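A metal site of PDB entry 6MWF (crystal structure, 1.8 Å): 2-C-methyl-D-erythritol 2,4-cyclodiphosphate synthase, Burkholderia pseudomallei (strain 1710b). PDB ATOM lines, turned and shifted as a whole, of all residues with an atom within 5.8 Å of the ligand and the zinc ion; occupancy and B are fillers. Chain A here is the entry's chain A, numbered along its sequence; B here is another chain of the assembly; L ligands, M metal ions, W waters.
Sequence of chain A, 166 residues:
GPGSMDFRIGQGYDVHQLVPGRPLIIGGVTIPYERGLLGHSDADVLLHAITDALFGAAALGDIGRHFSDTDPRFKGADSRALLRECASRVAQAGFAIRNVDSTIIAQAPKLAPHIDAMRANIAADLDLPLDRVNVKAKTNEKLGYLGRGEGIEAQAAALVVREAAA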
ATOM      1  N   TYR A  13      -7.667 -19.457 -16.766  1.00  0.00           N
ATOM      2  CA  TYR A  13      -7.950 -19.490 -18.187  1.00  0.00           C
ATOM      3  C   TYR A  13      -9.384 -19.958 -18.367  1.00  0.00           C
ATOM      4  O   TYR A  13      -9.816 -20.870 -17.661  1.00  0.00           O
ATOM      5  CB  TYR A  13      -6.997 -20.460 -18.919  1.00  0.00           C
ATOM      6  CG  TYR A  13      -7.436 -20.821 -20.330  1.00  0.00           C
ATOM      7  CD1 TYR A  13      -7.133 -19.979 -21.381  1.00  0.00           C
ATOM      8  CD2 TYR A  13      -8.162 -21.967 -20.596  1.00  0.00           C
ATOM      9  CE1 TYR A  13      -7.520 -20.270 -22.675  1.00  0.00           C
ATOM     10  CE2 TYR A  13      -8.568 -22.269 -21.896  1.00  0.00           C
ATOM     11  CZ  TYR A  13      -8.238 -21.415 -22.918  1.00  0.00           C
ATOM     12  OH  TYR A  13      -8.626 -21.706 -24.213  1.00  0.00           O
ATOM     13  N   ASP A  14     -10.107 -19.382 -19.327  1.00  0.00           N
ATOM     14  CA  ASP A  14     -11.387 -19.979 -19.668  1.00  0.00           C
ATOM     15  C   ASP A  14     -11.721 -19.627 -21.115  1.00  0.00           C
ATOM     16  O   ASP A  14     -11.250 -18.631 -21.657  1.00  0.00           O
ATOM     17  CB  ASP A  14     -12.490 -19.506 -18.721  1.00  0.00           C
ATOM     18  CG  ASP A  14     -13.742 -20.393 -18.779  1.00  0.00           C
ATOM     19  OD1 ASP A  14     -13.650 -21.554 -19.239  1.00  0.00           O
ATOM     20  OD2 ASP A  14     -14.830 -19.940 -18.375  1.00  0.00           O
ATOM     21  N   VAL A  15     -12.582 -20.447 -21.720  1.00  0.00           N
ATOM     22  CA  VAL A  15     -13.077 -20.178 -23.064  1.00  0.00           C
ATOM     23  C   VAL A  15     -14.500 -20.704 -23.145  1.00  0.00           C
ATOM     24  O   VAL A  15     -14.833 -21.715 -22.528  1.00  0.00           O
ATOM     25  CB  VAL A  15     -12.169 -20.821 -24.140  1.00  0.00           C
ATOM     26  CG1 VAL A  15     -12.195 -22.345 -24.065  1.00  0.00           C
ATOM     27  CG2 VAL A  15     -12.561 -20.322 -25.540  1.00  0.00           C
ATOM     28  N   HIS A  16     -15.358 -20.005 -23.894  1.00  0.00           N
ATOM     29  CA  HIS A  16     -16.693 -20.484 -24.201  1.00  0.00           C
ATOM     30  C   HIS A  16     -17.019 -20.189 -25.656  1.00  0.00           C
ATOM     31  O   HIS A  16     -16.601 -19.175 -26.211  1.00  0.00           O
ATOM     32  CB  HIS A  16     -17.771 -19.830 -23.293  1.00  0.00           C
ATOM     33  CG  HIS A  16     -17.767 -20.350 -21.885  1.00  0.00           C
ATOM     34  ND1 HIS A  16     -18.580 -21.381 -21.476  1.00  0.00           N
ATOM     35  CD2 HIS A  16     -17.044 -19.980 -20.799  1.00  0.00           C
ATOM     36  CE1 HIS A  16     -18.356 -21.625 -20.188  1.00  0.00           C
ATOM     37  NE2 HIS A  16     -17.429 -20.793 -19.761  1.00  0.00           N
ATOM     38  N   LEU A  38     -21.967 -19.924 -24.591  1.00  0.00           N
ATOM     39  CA  LEU A  38     -22.607 -21.199 -24.300  1.00  0.00           C
ATOM     40  C   LEU A  38     -21.948 -21.861 -23.089  1.00  0.00           C
ATOM     41  O   LEU A  38     -20.737 -22.077 -23.073  1.00  0.00           O
ATOM     42  CB  LEU A  38     -22.505 -22.141 -25.504  1.00  0.00           C
ATOM     43  CG  LEU A  38     -23.070 -23.537 -25.358  1.00  0.00           C
ATOM     44  CD1 LEU A  38     -24.589 -23.460 -25.284  1.00  0.00           C
ATOM     45  CD2 LEU A  38     -22.602 -24.383 -26.532  1.00  0.00           C
ATOM     46  N   GLY A  39     -22.774 -22.234 -22.111  1.00  0.00           N
ATOM     47  CA  GLY A  39     -22.262 -22.934 -20.956  1.00  0.00           C
ATOM     48  C   GLY A  39     -23.399 -23.375 -20.080  1.00  0.00           C
ATOM     49  O   GLY A  39     -24.567 -23.020 -20.308  1.00  0.00           O
ATOM     50  N   HIS A  40     -23.059 -24.191 -19.085  1.00  0.00           N
ATOM     51  CA  HIS A  40     -24.058 -24.665 -18.121  1.00  0.00           C
ATOM     52  C   HIS A  40     -24.572 -23.505 -17.263  1.00  0.00           C
ATOM     53  O   HIS A  40     -25.779 -23.358 -17.057  1.00  0.00           O
ATOM     54  CB  HIS A  40     -23.431 -25.762 -17.255  1.00  0.00           C
ATOM     55  CG  HIS A  40     -24.365 -26.374 -16.271  1.00  0.00           C
ATOM     56  ND1 HIS A  40     -25.502 -27.044 -16.652  1.00  0.00           N
ATOM     57  CD2 HIS A  40     -24.317 -26.444 -14.915  1.00  0.00           C
ATOM     58  CE1 HIS A  40     -26.132 -27.477 -15.569  1.00  0.00           C
ATOM     59  NE2 HIS A  40     -25.432 -27.128 -14.509  1.00  0.00           N
ATOM     60  N   SER A  41     -23.651 -22.671 -16.770  1.00  0.00           N
ATOM     61  CA  SER A  41     -23.977 -21.475 -16.017  1.00  0.00           C
ATOM     62  C   SER A  41     -24.315 -20.345 -16.983  1.00  0.00           C
ATOM     63  O   SER A  41     -24.581 -20.607 -18.160  1.00  0.00           O
ATOM     64  CB  SER A  41     -22.799 -21.073 -15.117  1.00  0.00           C
ATOM     65  OG  SER A  41     -21.719 -20.501 -15.873  1.00  0.00           O
ATOM     66  N   ASP A  42     -24.283 -19.095 -16.518  1.00  0.00           N
ATOM     67  CA  ASP A  42     -24.447 -18.015 -17.475  1.00  0.00           C
ATOM     68  C   ASP A  42     -23.239 -17.862 -18.389  1.00  0.00           C
ATOM     69  O   ASP A  42     -23.231 -16.975 -19.256  1.00  0.00           O
ATOM     70  CB  ASP A  42     -24.749 -16.693 -16.750  1.00  0.00           C
ATOM     71  CG  ASP A  42     -23.590 -16.173 -15.911  1.00  0.00           C
ATOM     72  OD1 ASP A  42     -22.453 -16.702 -15.987  1.00  0.00           O
ATOM     73  OD2 ASP A  42     -23.837 -15.210 -15.155  1.00  0.00           O
ATOM     74  N   ALA A  43     -22.217 -18.708 -18.219  1.00  0.00           N
ATOM     75  CA  ALA A  43     -21.091 -18.825 -19.142  1.00  0.00           C
ATOM     76  C   ALA A  43     -20.188 -17.592 -19.152  1.00  0.00           C
ATOM     77  O   ALA A  43     -19.548 -17.291 -20.171  1.00  0.00           O
ATOM     78  CB  ALA A  43     -21.554 -19.166 -20.564  1.00  0.00           C
ATOM     79  N   ASP A  44     -20.104 -16.886 -18.037  1.00  0.00           N
ATOM     80  CA  ASP A  44     -19.284 -15.686 -17.931  1.00  0.00           C
ATOM     81  C   ASP A  44     -17.806 -16.049 -17.898  1.00  0.00           C
ATOM     82  O   ASP A  44     -17.223 -16.331 -16.842  1.00  0.00           O
ATOM     83  CB  ASP A  44     -19.672 -14.882 -16.687  1.00  0.00           C
ATOM     84  CG  ASP A  44     -19.119 -13.465 -16.714  1.00  0.00           C
ATOM     85  OD1 ASP A  44     -17.970 -13.248 -17.188  1.00  0.00           O
ATOM     86  OD2 ASP A  44     -19.845 -12.565 -16.241  1.00  0.00           O
ATOM     87  N   VAL A  45     -17.194 -16.029 -19.091  1.00  0.00           N
ATOM     88  CA  VAL A  45     -15.834 -16.551 -19.264  1.00  0.00           C
ATOM     89  C   VAL A  45     -14.828 -15.732 -18.445  1.00  0.00           C
ATOM     90  O   VAL A  45     -13.828 -16.273 -17.934  1.00  0.00           O
ATOM     91  CB  VAL A  45     -15.516 -16.565 -20.773  1.00  0.00           C
ATOM     92  CG1 VAL A  45     -15.572 -15.162 -21.366  1.00  0.00           C
ATOM     93  CG2 VAL A  45     -14.172 -17.226 -21.072  1.00  0.00           C
ATOM     94  N   HIS A  48     -15.176 -16.617 -14.727  1.00  0.00           N
ATOM     95  CA  HIS A  48     -14.673 -17.966 -14.487  1.00  0.00           C
ATOM     96  C   HIS A  48     -13.147 -17.976 -14.434  1.00  0.00           C
ATOM     97  O   HIS A  48     -12.543 -18.663 -13.591  1.00  0.00           O
ATOM     98  CB  HIS A  48     -15.171 -18.944 -15.560  1.00  0.00           C
ATOM     99  CG  HIS A  48     -16.662 -19.127 -15.554  1.00  0.00           C
ATOM    100  ND1 HIS A  48     -17.334 -19.839 -16.509  1.00  0.00           N
ATOM    101  CD2 HIS A  48     -17.605 -18.694 -14.671  1.00  0.00           C
ATOM    102  CE1 HIS A  48     -18.630 -19.826 -16.257  1.00  0.00           C
ATOM    103  NE2 HIS A  48     -18.823 -19.135 -15.145  1.00  0.00           N
ATOM    104  N   ASP A  52     -10.959 -19.086 -11.170  1.00  0.00           N
ATOM    105  CA  ASP A  52      -9.915 -20.112 -11.204  1.00  0.00           C
ATOM    106  C   ASP A  52      -8.596 -19.577 -10.661  1.00  0.00           C
ATOM    107  O   ASP A  52      -7.871 -20.292  -9.953  1.00  0.00           O
ATOM    108  CB  ASP A  52      -9.737 -20.640 -12.634  1.00  0.00           C
ATOM    109  CG  ASP A  52     -10.214 -22.071 -12.804  1.00  0.00           C
ATOM    110  OD1 ASP A  52     -10.896 -22.576 -11.898  1.00  0.00           O
ATOM    111  OD2 ASP A  52      -9.918 -22.727 -13.848  1.00  0.00           O
ATOM    112  N   ILE A  63     -12.561 -24.206 -10.387  1.00  0.00           N
ATOM    113  CA  ILE A  63     -13.990 -23.942 -10.400  1.00  0.00           C
ATOM    114  C   ILE A  63     -14.779 -25.229 -10.607  1.00  0.00           C
ATOM    115  O   ILE A  63     -15.860 -25.398 -10.029  1.00  0.00           O
ATOM    116  CB  ILE A  63     -14.269 -22.851 -11.466  1.00  0.00           C
ATOM    117  CG1 ILE A  63     -15.684 -22.312 -11.335  1.00  0.00           C
ATOM    118  CG2 ILE A  63     -14.026 -23.387 -12.870  1.00  0.00           C
ATOM    119  CD1 ILE A  63     -15.955 -21.118 -12.271  1.00  0.00           C
ATOM    120  N   GLY A  64     -14.240 -26.178 -11.372  1.00  0.00           N
ATOM    121  CA  GLY A  64     -14.907 -27.460 -11.521  1.00  0.00           C
ATOM    122  C   GLY A  64     -15.028 -28.224 -10.212  1.00  0.00           C
ATOM    123  O   GLY A  64     -16.021 -28.900  -9.969  1.00  0.00           O
ATOM    124  N   PHE A  67     -17.764 -25.935  -8.042  1.00  0.00           N
ATOM    125  CA  PHE A  67     -19.082 -25.709  -8.627  1.00  0.00           C
ATOM    126  C   PHE A  67     -19.191 -26.551  -9.908  1.00  0.00           C
ATOM    127  O   PHE A  67     -19.006 -26.041 -11.026  1.00  0.00           O
ATOM    128  CB  PHE A  67     -19.332 -24.237  -8.942  1.00  0.00           C
ATOM    129  CG  PHE A  67     -18.889 -23.255  -7.885  1.00  0.00           C
ATOM    130  CD1 PHE A  67     -19.563 -23.139  -6.666  1.00  0.00           C
ATOM    131  CD2 PHE A  67     -17.872 -22.341  -8.167  1.00  0.00           C
ATOM    132  CE1 PHE A  67     -19.181 -22.187  -5.734  1.00  0.00           C
ATOM    133  CE2 PHE A  67     -17.479 -21.379  -7.222  1.00  0.00           C
ATOM    134  CZ  PHE A  67     -18.129 -21.302  -6.009  1.00  0.00           C
ATOM    135  N   SER A  68     -19.529 -27.828  -9.763  1.00  0.00           N
ATOM    136  CA  SER A  68     -19.489 -28.746 -10.900  1.00  0.00           C
ATOM    137  C   SER A  68     -20.453 -28.320 -12.008  1.00  0.00           C
ATOM    138  O   SER A  68     -21.612 -27.984 -11.729  1.00  0.00           O
ATOM    139  CB  SER A  68     -19.813 -30.165 -10.437  1.00  0.00           C
ATOM    140  OG  SER A  68     -21.169 -30.254 -10.033  1.00  0.00           O
ATOM    141  N   ASP A  69     -19.973 -28.356 -13.256  1.00  0.00           N
ATOM    142  CA  ASP A  69     -20.831 -28.063 -14.402  1.00  0.00           C
ATOM    143  C   ASP A  69     -21.842 -29.165 -14.664  1.00  0.00           C
ATOM    144  O   ASP A  69     -22.690 -29.008 -15.555  1.00  0.00           O
ATOM    145  CB  ASP A  69     -19.986 -27.833 -15.659  1.00  0.00           C
ATOM    146  N   THR A  70     -21.771 -30.276 -13.941  1.00  0.00           N
ATOM    147  CA  THR A  70     -22.789 -31.310 -14.032  1.00  0.00           C
ATOM    148  C   THR A  70     -23.965 -31.053 -13.113  1.00  0.00           C
ATOM    149  O   THR A  70     -25.027 -31.649 -13.308  1.00  0.00           O
ATOM    150  CB  THR A  70     -22.167 -32.681 -13.711  1.00  0.00           C
ATOM    151  N   PHE A  74     -26.554 -25.315 -10.667  1.00  0.00           N
ATOM    152  CA  PHE A  74     -25.797 -24.259 -11.296  1.00  0.00           C
ATOM    153  C   PHE A  74     -26.224 -23.997 -12.728  1.00  0.00           C
ATOM    154  O   PHE A  74     -25.569 -23.218 -13.419  1.00  0.00           O
ATOM    155  CB  PHE A  74     -24.292 -24.593 -11.248  1.00  0.00           C
ATOM    156  CG  PHE A  74     -23.745 -24.705  -9.856  1.00  0.00           C
ATOM    157  CD1 PHE A  74     -23.177 -25.896  -9.409  1.00  0.00           C
ATOM    158  CD2 PHE A  74     -23.802 -23.636  -8.980  1.00  0.00           C
ATOM    159  CE1 PHE A  74     -22.680 -26.006  -8.130  1.00  0.00           C
ATOM    160  CE2 PHE A  74     -23.312 -23.746  -7.694  1.00  0.00           C
ATOM    161  CZ  PHE A  74     -22.752 -24.938  -7.271  1.00  0.00           C
ATOM    162  N   ALA A  77     -26.523 -20.422 -13.603  1.00  0.00           N
ATOM    163  CA  ALA A  77     -26.050 -19.711 -12.420  1.00  0.00           C
ATOM    164  C   ALA A  77     -25.447 -18.369 -12.763  1.00  0.00           C
ATOM    165  O   ALA A  77     -24.738 -18.215 -13.758  1.00  0.00           O
ATOM    166  CB  ALA A  77     -25.018 -20.556 -11.667  1.00  0.00           C
ATOM    167  N   SER A  79     -22.713 -15.982 -12.464  1.00  0.00           N
ATOM    168  CA  SER A  79     -21.318 -16.211 -12.134  1.00  0.00           C
ATOM    169  C   SER A  79     -20.753 -15.161 -11.178  1.00  0.00           C
ATOM    170  O   SER A  79     -19.660 -15.386 -10.643  1.00  0.00           O
ATOM    171  CB  SER A  79     -20.479 -16.269 -13.407  1.00  0.00           C
ATOM    172  OG  SER A  79     -20.823 -17.450 -14.146  1.00  0.00           O
ATOM    173  N   LEU A  82     -21.180 -16.943  -7.975  1.00  0.00           N
ATOM    174  CA  LEU A  82     -20.117 -17.931  -7.854  1.00  0.00           C
ATOM    175  C   LEU A  82     -18.795 -17.267  -7.479  1.00  0.00           C
ATOM    176  O   LEU A  82     -18.047 -17.783  -6.652  1.00  0.00           O
ATOM    177  CB  LEU A  82     -19.964 -18.708  -9.159  1.00  0.00           C
ATOM    178  CG  LEU A  82     -21.183 -19.521  -9.634  1.00  0.00           C
ATOM    179  CD1 LEU A  82     -20.846 -20.240 -10.930  1.00  0.00           C
ATOM    180  CD2 LEU A  82     -21.637 -20.498  -8.559  1.00  0.00           C
ATOM    181  N   LYS B 138      -9.137 -28.232 -17.348  1.00  0.00           N
ATOM    182  CA  LYS B 138     -10.372 -27.955 -18.062  1.00  0.00           C
ATOM    183  C   LYS B 138     -10.247 -28.374 -19.515  1.00  0.00           C
ATOM    184  O   LYS B 138      -9.188 -28.724 -20.006  1.00  0.00           O
ATOM    185  CB  LYS B 138     -10.751 -26.493 -17.988  1.00  0.00           C
ATOM    186  CG  LYS B 138      -9.805 -25.553 -18.726  1.00  0.00           C
ATOM    187  CD  LYS B 138      -9.693 -24.235 -17.982  1.00  0.00           C
ATOM    188  CE  LYS B 138     -10.872 -24.004 -17.038  1.00  0.00           C
ATOM    189  NZ  LYS B 138     -12.141 -23.703 -17.773  1.00  0.00           N
ATOM    190  N   GLU B 141     -13.691 -26.598 -24.691  1.00  0.00           N
ATOM    191  CA  GLU B 141     -15.034 -26.417 -25.247  1.00  0.00           C
ATOM    192  C   GLU B 141     -15.066 -26.754 -26.733  1.00  0.00           C
ATOM    193  O   GLU B 141     -15.751 -26.107 -27.533  1.00  0.00           O
ATOM    194  CB  GLU B 141     -15.549 -24.985 -24.995  1.00  0.00           C
ATOM    195  CG  GLU B 141     -15.817 -24.683 -23.539  1.00  0.00           C
ATOM    196  CD  GLU B 141     -16.966 -25.475 -22.969  1.00  0.00           C
ATOM    197  OE1 GLU B 141     -18.057 -25.527 -23.585  1.00  0.00           O
ATOM    198  OE2 GLU B 141     -16.779 -26.078 -21.895  1.00  0.00           O
HETATM  199  O1  LIG L   1     -20.881 -22.415 -17.675  1.00  0.00           O
HETATM  200  S1  LIG L   1     -19.858 -23.502 -17.190  1.00  0.00           S
HETATM  201  O2  LIG L   1     -19.893 -24.963 -17.798  1.00  0.00           O
HETATM  202  C1  LIG L   1     -20.126 -23.629 -15.426  1.00  0.00           C
HETATM  203  C2  LIG L   1     -19.556 -22.729 -14.559  1.00  0.00           C
HETATM  204  C3  LIG L   1     -19.814 -22.837 -13.210  1.00  0.00           C
HETATM  205  C4  LIG L   1     -20.685 -23.830 -12.731  1.00  0.00           C
HETATM  206  N1  LIG L   1     -20.970 -23.949 -11.411  1.00  0.00           N
HETATM  207  C5  LIG L   1     -21.276 -24.701 -13.649  1.00  0.00           C
HETATM  208  C6  LIG L   1     -21.009 -24.596 -14.988  1.00  0.00           C
HETATM  209  N2  LIG L   1     -18.275 -22.858 -17.269  1.00  0.00           N
HETATM  210  C7  LIG L   1     -17.124 -23.471 -16.805  1.00  0.00           C
HETATM  211  C8  LIG L   1     -17.125 -24.716 -16.193  1.00  0.00           C
HETATM  212  C9  LIG L   1     -15.921 -25.219 -15.771  1.00  0.00           C
HETATM  213  C10 LIG L   1     -14.760 -24.486 -15.963  1.00  0.00           C
HETATM  214  C11 LIG L   1     -14.863 -23.247 -16.569  1.00  0.00           C
HETATM  215  N3  LIG L   1     -16.028 -22.764 -16.995  1.00  0.00           N
HETATM  216 ZN    ZN M   1     -16.489 -20.919 -17.962  1.00  0.00          ZN
HETATM  217  O   HOH W   1     -19.403 -25.154 -20.979  1.00  0.00           O
HETATM  218  O   HOH W   2     -16.853 -28.175 -14.448  1.00  0.00           O
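An oxygen (O1) of the ligand lies within hydrogen-bond range of the backbone NH (N) of Ser 41, at 2.9 Å. The backbone carbonyl oxygen (O) of Phe 67 sits at hydrogen-bond distance from a nitrogen (N1) of the ligand, at 2.9 Å. N of His 40 sits at hydrogen-bond distance from O1 of the ligand (3.1 Å). OG of Ser 41 lies within hydrogen-bond range of O1 of the ligand.
The side-chain amino group of Lys 138 of chain B is in salt-bridge range of the side-chain carboxylate of Asp 14, 3.0 Å away. The side-chain hydroxyl of Ser 41 sits close to the backbone NH of Ala 43, 3.0 Å away. The backbone carbonyl oxygen (O) of Leu 38 is in hydrogen-bond range of a ring nitrogen (ND1) of His 16 (2.8 Å). A ring nitrogen (NE2) of His 48 sits close to the side-chain hydroxyl of Ser 41 (3.3 Å). A ring nitrogen (NE2) of His 40 lies close to the backbone carbonyl oxygen (O) of Asp 69, at 3.5 Å. NE2 of His 48 sits at hydrogen-bond distance from OG of Ser 79 (2.8 Å). The backbone NH (N) of Ile 63 is in hydrogen-bond range of the side-chain carboxylate (OD1) of Asp 52 (2.8 Å).
Gly 39 touches the ligand. CA of Ala 43 touches O1 of the ligand, at 3.9 Å. Ile 63 touches the ligand. Ser 68 touches the ligand (O to C5, 3.8 Å). Asp 69 touches the ligand. CG of Phe 74 touches N1 of the ligand (3.3 Å). Leu 82 touches the ligand (CD1 to C3, 3.6 Å). Lys 138 of chain B touches the ligand (NZ to C11, 3.0 Å). Hydrophobic or aromatic side chains within 4 Å of the ligand: His 16, His 40, His 48, Ile 63, Phe 67, Phe 74 and Leu 82. Within 4 Å of the ligand: Asp 14, His 16, Gly 39, His 40, Ser 41, Ala 43, His 48, Ile 63, Phe 67, Ser 68, Asp 69, Phe 74, Leu 82 and Lys 138 of chain B. The nearest printed residue that does not touch the ligand is Gly 64 (4.8 Å).
Within 4 Å of the zinc ion: Asp 14, His 16 and His 48.
The zinc ion is bound by OD2 of Asp 14, ND1 of His 48, NE2 of His 16 and N3 of the ligand. The zinc ion has four donor atoms within binding distance. Slightly farther from the zinc ion lies a nitrogen (N2) of the ligand (2.7 Å).
Water W1 lies within hydrogen-bond range of OE2 of Glu 141 of chain B (2.9 Å) and O2 of the ligand (3.2 Å).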
